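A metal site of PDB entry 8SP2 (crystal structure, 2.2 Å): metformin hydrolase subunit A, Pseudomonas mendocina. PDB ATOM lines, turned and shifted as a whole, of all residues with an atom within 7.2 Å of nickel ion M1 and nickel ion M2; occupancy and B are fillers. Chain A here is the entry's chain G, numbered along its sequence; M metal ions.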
ATOM      1  N   ASP A 158       6.668   3.068  13.678  1.00  0.00           N
ATOM      2  CA  ASP A 158       8.093   3.372  13.621  1.00  0.00           C
ATOM      3  C   ASP A 158       8.344   4.798  13.097  1.00  0.00           C
ATOM      4  O   ASP A 158       7.430   5.514  12.676  1.00  0.00           O
ATOM      5  CB  ASP A 158       8.841   2.324  12.797  1.00  0.00           C
ATOM      6  CG  ASP A 158       8.470   2.332  11.323  1.00  0.00           C
ATOM      7  OD1 ASP A 158       8.487   3.428  10.753  1.00  0.00           O
ATOM      8  OD2 ASP A 158       8.202   1.245  10.757  1.00  0.00           O
ATOM      9  N   HIS A 159       9.617   5.209  13.121  1.00  0.00           N
ATOM     10  CA  HIS A 159       9.964   6.585  12.818  1.00  0.00           C
ATOM     11  C   HIS A 159      10.089   6.857  11.321  1.00  0.00           C
ATOM     12  O   HIS A 159      10.646   7.881  10.956  1.00  0.00           O
ATOM     13  CB  HIS A 159      11.296   6.980  13.461  1.00  0.00           C
ATOM     14  CG  HIS A 159      11.305   8.427  13.814  1.00  0.00           C
ATOM     15  ND1 HIS A 159      12.296   8.995  14.576  1.00  0.00           N
ATOM     16  CD2 HIS A 159      10.409   9.373  13.589  1.00  0.00           C
ATOM     17  CE1 HIS A 159      11.989  10.273  14.764  1.00  0.00           C
ATOM     18  NE2 HIS A 159      10.846  10.529  14.176  1.00  0.00           N
ATOM     19  N   SER A 160       9.567   5.963  10.462  1.00  0.00           N
ATOM     20  CA  SER A 160       9.351   6.310   9.065  1.00  0.00           C
ATOM     21  C   SER A 160       8.227   7.342   8.979  1.00  0.00           C
ATOM     22  O   SER A 160       8.087   8.030   7.960  1.00  0.00           O
ATOM     23  CB  SER A 160       9.060   5.091   8.208  1.00  0.00           C
ATOM     24  OG  SER A 160       7.770   4.553   8.470  1.00  0.00           O
ATOM     25  N   PRO A 162       7.541  10.456   9.897  1.00  0.00           N
ATOM     26  CA  PRO A 162       7.774  11.808   9.360  1.00  0.00           C
ATOM     27  C   PRO A 162       7.980  11.942   7.840  1.00  0.00           C
ATOM     28  O   PRO A 162       7.833  13.039   7.282  1.00  0.00           O
ATOM     29  CB  PRO A 162       9.035  12.307  10.085  1.00  0.00           C
ATOM     30  CG  PRO A 162       9.687  11.080  10.680  1.00  0.00           C
ATOM     31  CD  PRO A 162       8.549  10.104  10.903  1.00  0.00           C
ATOM     32  N   HIS A 182      12.902  17.736  14.885  1.00  0.00           N
ATOM     33  CA  HIS A 182      13.102  16.317  15.117  1.00  0.00           C
ATOM     34  C   HIS A 182      13.718  16.085  16.489  1.00  0.00           C
ATOM     35  O   HIS A 182      14.886  16.393  16.705  1.00  0.00           O
ATOM     36  CB  HIS A 182      14.041  15.760  14.036  1.00  0.00           C
ATOM     37  CG  HIS A 182      14.108  14.269  13.926  1.00  0.00           C
ATOM     38  ND1 HIS A 182      13.474  13.588  12.910  1.00  0.00           N
ATOM     39  CD2 HIS A 182      14.733  13.342  14.662  1.00  0.00           C
ATOM     40  CE1 HIS A 182      13.710  12.286  13.044  1.00  0.00           C
ATOM     41  NE2 HIS A 182      14.480  12.116  14.086  1.00  0.00           N
ATOM     42  N   VAL A 183      12.952  15.497  17.413  1.00  0.00           N
ATOM     43  CA  VAL A 183      13.448  15.281  18.769  1.00  0.00           C
ATOM     44  C   VAL A 183      13.591  13.774  18.979  1.00  0.00           C
ATOM     45  O   VAL A 183      12.618  13.037  18.860  1.00  0.00           O
ATOM     46  CB  VAL A 183      12.539  15.932  19.819  1.00  0.00           C
ATOM     47  CG1 VAL A 183      12.966  15.581  21.247  1.00  0.00           C
ATOM     48  CG2 VAL A 183      12.474  17.436  19.647  1.00  0.00           C
ATOM     49  N   ASP A 184      14.807  13.350  19.297  1.00  0.00           N
ATOM     50  CA  ASP A 184      15.196  11.959  19.140  1.00  0.00           C
ATOM     51  C   ASP A 184      16.582  11.800  19.760  1.00  0.00           C
ATOM     52  O   ASP A 184      17.336  12.753  19.793  1.00  0.00           O
ATOM     53  CB  ASP A 184      15.172  11.605  17.654  1.00  0.00           C
ATOM     54  CG  ASP A 184      15.087  10.125  17.304  1.00  0.00           C
ATOM     55  OD1 ASP A 184      15.443   9.270  18.169  1.00  0.00           O
ATOM     56  OD2 ASP A 184      14.649   9.831  16.160  1.00  0.00           O
ATOM     57  N   CYS A 185      16.852  10.598  20.289  1.00  0.00           N
ATOM     58  CA  CYS A 185      18.177  10.138  20.668  1.00  0.00           C
ATOM     59  C   CYS A 185      19.069   9.903  19.446  1.00  0.00           C
ATOM     60  O   CYS A 185      20.304   9.952  19.526  1.00  0.00           O
ATOM     61  CB  CYS A 185      18.059   8.791  21.371  1.00  0.00           C
ATOM     62  SG  CYS A 185      19.629   8.185  22.030  1.00  0.00           S
ATOM     63  N   HIS A 186      18.416   9.538  18.343  1.00  0.00           N
ATOM     64  CA  HIS A 186      19.063   9.150  17.098  1.00  0.00           C
ATOM     65  C   HIS A 186      18.945  10.314  16.129  1.00  0.00           C
ATOM     66  O   HIS A 186      17.911  10.967  16.041  1.00  0.00           O
ATOM     67  CB  HIS A 186      18.406   7.886  16.537  1.00  0.00           C
ATOM     68  CG  HIS A 186      18.289   6.781  17.537  1.00  0.00           C
ATOM     69  ND1 HIS A 186      17.102   6.269  18.038  1.00  0.00           N
ATOM     70  CD2 HIS A 186      19.273   6.133  18.187  1.00  0.00           C
ATOM     71  CE1 HIS A 186      17.379   5.326  18.916  1.00  0.00           C
ATOM     72  NE2 HIS A 186      18.684   5.227  19.027  1.00  0.00           N
ATOM     73  N   LEU A 187      20.021  10.531  15.367  1.00  0.00           N
ATOM     74  CA  LEU A 187      20.112  11.645  14.450  1.00  0.00           C
ATOM     75  C   LEU A 187      19.235  11.444  13.204  1.00  0.00           C
ATOM     76  O   LEU A 187      18.760  12.424  12.641  1.00  0.00           O
ATOM     77  CB  LEU A 187      21.596  11.842  14.099  1.00  0.00           C
ATOM     78  CG  LEU A 187      22.451  12.458  15.209  1.00  0.00           C
ATOM     79  CD1 LEU A 187      23.913  12.460  14.809  1.00  0.00           C
ATOM     80  CD2 LEU A 187      21.997  13.884  15.538  1.00  0.00           C
ATOM     81  N   ASP A 188      19.009  10.182  12.793  1.00  0.00           N
ATOM     82  CA  ASP A 188      18.069   9.849  11.720  1.00  0.00           C
ATOM     83  C   ASP A 188      18.344  10.660  10.446  1.00  0.00           C
ATOM     84  O   ASP A 188      17.430  11.271   9.890  1.00  0.00           O
ATOM     85  CB  ASP A 188      16.614  10.086  12.159  1.00  0.00           C
ATOM     86  CG  ASP A 188      16.027   9.049  13.113  1.00  0.00           C
ATOM     87  OD1 ASP A 188      16.783   8.228  13.629  1.00  0.00           O
ATOM     88  OD2 ASP A 188      14.793   9.000  13.229  1.00  0.00           O
ATOM     89  N   ASN A 200      13.213   4.286   8.687  1.00  0.00           N
ATOM     90  CA  ASN A 200      12.856   5.124   9.823  1.00  0.00           C
ATOM     91  C   ASN A 200      14.036   5.961  10.295  1.00  0.00           C
ATOM     92  O   ASN A 200      13.872   6.776  11.197  1.00  0.00           O
ATOM     93  CB  ASN A 200      12.320   4.298  10.992  1.00  0.00           C
ATOM     94  CG  ASN A 200      13.358   3.416  11.672  1.00  0.00           C
ATOM     95  OD1 ASN A 200      14.333   2.976  11.074  1.00  0.00           O
ATOM     96  ND2 ASN A 200      13.102   3.107  12.936  1.00  0.00           N
ATOM     97  N   CYS A 201      15.215   5.769   9.680  1.00  0.00           N
ATOM     98  CA  CYS A 201      16.364   6.568  10.060  1.00  0.00           C
ATOM     99  C   CYS A 201      16.785   7.557   8.965  1.00  0.00           C
ATOM    100  O   CYS A 201      17.968   7.865   8.836  1.00  0.00           O
ATOM    101  CB  CYS A 201      17.523   5.653  10.433  1.00  0.00           C
ATOM    102  SG  CYS A 201      18.049   4.611   9.049  1.00  0.00           S
ATOM    103  N   SER A 202      15.819   8.142   8.257  1.00  0.00           N
ATOM    104  CA  SER A 202      16.124   9.122   7.205  1.00  0.00           C
ATOM    105  C   SER A 202      15.088  10.241   7.183  1.00  0.00           C
ATOM    106  O   SER A 202      14.936  10.921   6.160  1.00  0.00           O
ATOM    107  CB  SER A 202      16.220   8.478   5.850  1.00  0.00           C
ATOM    108  OG  SER A 202      17.326   7.591   5.819  1.00  0.00           O
ATOM    109  N   HIS A 220      17.370  19.600  15.195  1.00  0.00           N
ATOM    110  CA  HIS A 220      17.334  18.338  15.907  1.00  0.00           C
ATOM    111  C   HIS A 220      17.658  18.562  17.383  1.00  0.00           C
ATOM    112  O   HIS A 220      18.500  19.391  17.699  1.00  0.00           O
ATOM    113  CB  HIS A 220      18.297  17.341  15.255  1.00  0.00           C
ATOM    114  CG  HIS A 220      18.203  15.945  15.778  1.00  0.00           C
ATOM    115  ND1 HIS A 220      18.561  15.597  17.048  1.00  0.00           N
ATOM    116  CD2 HIS A 220      17.816  14.805  15.172  1.00  0.00           C
ATOM    117  CE1 HIS A 220      18.417  14.286  17.202  1.00  0.00           C
ATOM    118  NE2 HIS A 220      17.949  13.782  16.087  1.00  0.00           N
ATOM    119  N   LEU A 227      24.403   4.903  18.842  1.00  0.00           N
ATOM    120  CA  LEU A 227      23.681   4.441  17.666  1.00  0.00           C
ATOM    121  C   LEU A 227      23.422   5.646  16.770  1.00  0.00           C
ATOM    122  O   LEU A 227      22.286   6.098  16.622  1.00  0.00           O
ATOM    123  CB  LEU A 227      22.377   3.727  18.022  1.00  0.00           C
ATOM    124  CG  LEU A 227      21.697   3.018  16.840  1.00  0.00           C
ATOM    125  CD1 LEU A 227      22.185   1.578  16.714  1.00  0.00           C
ATOM    126  CD2 LEU A 227      20.181   3.066  16.949  1.00  0.00           C
ATOM    127  N   TRP A 232      25.170  10.487   9.736  1.00  0.00           N
ATOM    128  CA  TRP A 232      23.970  11.137  10.253  1.00  0.00           C
ATOM    129  C   TRP A 232      24.371  12.486  10.829  1.00  0.00           C
ATOM    130  O   TRP A 232      23.692  13.471  10.591  1.00  0.00           O
ATOM    131  CB  TRP A 232      23.249  10.281  11.300  1.00  0.00           C
ATOM    132  CG  TRP A 232      22.745   8.955  10.826  1.00  0.00           C
ATOM    133  CD1 TRP A 232      22.931   8.382   9.605  1.00  0.00           C
ATOM    134  CD2 TRP A 232      21.988   8.016  11.605  1.00  0.00           C
ATOM    135  NE1 TRP A 232      22.328   7.148   9.566  1.00  0.00           N
ATOM    136  CE2 TRP A 232      21.747   6.902  10.784  1.00  0.00           C
ATOM    137  CE3 TRP A 232      21.493   8.000  12.921  1.00  0.00           C
ATOM    138  CZ2 TRP A 232      21.028   5.784  11.233  1.00  0.00           C
ATOM    139  CZ3 TRP A 232      20.788   6.908  13.358  1.00  0.00           C
ATOM    140  CH2 TRP A 232      20.549   5.813  12.522  1.00  0.00           C
ATOM    141  N   THR A 275       8.269  15.998  14.788  1.00  0.00           N
ATOM    142  CA  THR A 275       8.323  14.572  15.069  1.00  0.00           C
ATOM    143  C   THR A 275       9.098  14.313  16.367  1.00  0.00           C
ATOM    144  O   THR A 275      10.192  14.841  16.554  1.00  0.00           O
ATOM    145  CB  THR A 275       8.973  13.778  13.923  1.00  0.00           C
ATOM    146  OG1 THR A 275       8.913  12.370  14.197  1.00  0.00           O
ATOM    147  CG2 THR A 275      10.415  14.169  13.681  1.00  0.00           C
ATOM    148  N   ASP A 277      10.405  11.246  18.873  1.00  0.00           N
ATOM    149  CA  ASP A 277      10.684   9.853  19.184  1.00  0.00           C
ATOM    150  C   ASP A 277      10.732   9.643  20.700  1.00  0.00           C
ATOM    151  O   ASP A 277      11.447  10.349  21.411  1.00  0.00           O
ATOM    152  CB  ASP A 277      12.005   9.437  18.560  1.00  0.00           C
ATOM    153  CG  ASP A 277      12.188   7.945  18.395  1.00  0.00           C
ATOM    154  OD1 ASP A 277      11.714   7.178  19.276  1.00  0.00           O
ATOM    155  OD2 ASP A 277      12.827   7.542  17.378  1.00  0.00           O
ATOM    156  N   THR A 278      10.002   8.638  21.172  1.00  0.00           N
ATOM    157  CA  THR A 278       9.930   8.360  22.605  1.00  0.00           C
ATOM    158  C   THR A 278      11.273   7.847  23.134  1.00  0.00           C
ATOM    159  O   THR A 278      11.486   7.813  24.354  1.00  0.00           O
ATOM    160  CB  THR A 278       8.754   7.432  22.923  1.00  0.00           C
ATOM    161  OG1 THR A 278       8.829   6.257  22.118  1.00  0.00           O
ATOM    162  CG2 THR A 278       7.419   8.095  22.667  1.00  0.00           C
ATOM    163  N   ASP A 279      12.246   7.543  22.259  1.00  0.00           N
ATOM    164  CA  ASP A 279      13.549   7.248  22.822  1.00  0.00           C
ATOM    165  C   ASP A 279      14.360   8.515  23.085  1.00  0.00           C
ATOM    166  O   ASP A 279      15.505   8.436  23.540  1.00  0.00           O
ATOM    167  CB  ASP A 279      14.347   6.281  21.979  1.00  0.00           C
ATOM    168  CG  ASP A 279      14.581   6.844  20.606  1.00  0.00           C
ATOM    169  OD1 ASP A 279      14.724   8.101  20.508  1.00  0.00           O
ATOM    170  OD2 ASP A 279      14.557   6.024  19.673  1.00  0.00           O
ATOM    171  N   SER A 280      13.789   9.692  22.859  1.00  0.00           N
ATOM    172  CA  SER A 280      14.349  10.893  23.484  1.00  0.00           C
ATOM    173  C   SER A 280      14.213  10.822  25.013  1.00  0.00           C
ATOM    174  O   SER A 280      15.011  11.407  25.743  1.00  0.00           O
ATOM    175  CB  SER A 280      13.712  12.110  22.918  1.00  0.00           C
ATOM    176  OG  SER A 280      12.322  12.179  23.208  1.00  0.00           O
ATOM    177  N   ASN A 289      10.324   0.761  24.296  1.00  0.00           N
ATOM    178  CA  ASN A 289      10.797   1.409  23.086  1.00  0.00           C
ATOM    179  C   ASN A 289      11.474   0.392  22.182  1.00  0.00           C
ATOM    180  O   ASN A 289      11.959  -0.630  22.641  1.00  0.00           O
ATOM    181  CB  ASN A 289      11.727   2.569  23.416  1.00  0.00           C
ATOM    182  CG  ASN A 289      11.822   3.541  22.277  1.00  0.00           C
ATOM    183  OD1 ASN A 289      12.747   3.466  21.462  1.00  0.00           O
ATOM    184  ND2 ASN A 289      10.857   4.437  22.192  1.00  0.00           N
ATOM    185  N   ALA A 291      14.235   1.037  20.616  1.00  0.00           N
ATOM    186  CA  ALA A 291      15.664   1.188  20.860  1.00  0.00           C
ATOM    187  C   ALA A 291      15.864   2.143  22.020  1.00  0.00           C
ATOM    188  O   ALA A 291      16.225   3.299  21.814  1.00  0.00           O
ATOM    189  CB  ALA A 291      16.341   1.715  19.625  1.00  0.00           C
ATOM    190  N   GLU A 293      17.159   4.201  25.411  1.00  0.00           N
ATOM    191  CA  GLU A 293      18.465   4.774  25.692  1.00  0.00           C
ATOM    192  C   GLU A 293      18.455   5.499  27.032  1.00  0.00           C
ATOM    193  O   GLU A 293      17.573   6.316  27.284  1.00  0.00           O
ATOM    194  CB  GLU A 293      18.805   5.789  24.604  1.00  0.00           C
ATOM    195  CG  GLU A 293      19.065   5.180  23.243  1.00  0.00           C
ATOM    196  CD  GLU A 293      20.473   4.635  23.066  1.00  0.00           C
ATOM    197  OE1 GLU A 293      21.160   4.389  24.109  1.00  0.00           O
ATOM    198  OE2 GLU A 293      20.884   4.486  21.893  1.00  0.00           O
ATOM    199  N   VAL A 320       6.491   8.707  17.998  1.00  0.00           N
ATOM    200  CA  VAL A 320       6.814   7.409  17.398  1.00  0.00           C
ATOM    201  C   VAL A 320       7.538   6.499  18.400  1.00  0.00           C
ATOM    202  O   VAL A 320       8.031   6.952  19.440  1.00  0.00           O
ATOM    203  CB  VAL A 320       7.674   7.560  16.119  1.00  0.00           C
ATOM    204  CG1 VAL A 320       7.037   8.519  15.130  1.00  0.00           C
ATOM    205  CG2 VAL A 320       9.090   8.005  16.428  1.00  0.00           C
ATOM    206  N   GLU A 321       7.571   5.209  18.009  1.00  0.00           N
ATOM    207  CA  GLU A 321       8.428   4.136  18.509  1.00  0.00           C
ATOM    208  C   GLU A 321       8.042   3.656  19.909  1.00  0.00           C
ATOM    209  O   GLU A 321       8.854   2.966  20.524  1.00  0.00           O
ATOM    210  CB  GLU A 321       9.921   4.497  18.428  1.00  0.00           C
ATOM    211  CG  GLU A 321      10.450   4.735  16.998  1.00  0.00           C
ATOM    212  CD  GLU A 321      10.716   3.526  16.091  1.00  0.00           C
ATOM    213  OE1 GLU A 321      10.431   2.385  16.507  1.00  0.00           O
ATOM    214  OE2 GLU A 321      11.205   3.742  14.919  1.00  0.00           O
HETATM  215 NI    NI M   1      15.083   7.066  17.847  1.00  0.00          NI
HETATM  216 NI    NI M   2      14.177   8.008  15.190  1.00  0.00          NI
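Nickel ion M2 is bound by OD2 of Asp 184, ND1 of His 159 and OD2 of Asp 188.
Nickel ion M2 has three donor atoms within binding distance.
Slightly farther from nickel ion M2 lies the side-chain carboxylate (OD2) of Asp 277 (2.6 Å).
Along chain A the residues within 4 Å of nickel ion M1 span positions 184 to 279.
The side-chain carboxylate of Asp 184 sits close to a ring nitrogen (NE2) of His 182 (3.1 Å).
The side-chain carboxylate of Asp 279 sits at hydrogen-bond distance from the backbone NH of Cys 185.
N of Asp 279 sits close to ND2 of Asn 289 (3.4 Å).
The backbone carbonyl oxygen (O) of His 186 lies within hydrogen-bond range of a ring nitrogen (NE2) of His 220.
The backbone NH (N) of His 159 sits at hydrogen-bond distance from the side-chain carboxylate (OE2) of Glu 321, 2.8 Å away.
NE2 of His 159 is in hydrogen-bond range of OG1 of Thr 275, at 2.7 Å.
The side-chain carboxylate (OD2) of Asp 188 lies close to a ring nitrogen (NE2) of His 182, 3.2 Å away.
The backbone NH (N) of Asp 277 is in hydrogen-bond range of the backbone carbonyl oxygen (O) of Val 183 (2.8 Å).
Nickel ion M1 is bound by the side-chain carboxylate (OD2) of Asp 279, a ring nitrogen (ND1) of His 186, the side-chain carboxylate (OD1) of Asp 184 and the side-chain carboxylate (OD2) of Asp 277.
Nickel ion M1 has four donor atoms within binding distance.
Of the 27 residues printed, 4 come within 4 Å of nickel ion M2.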
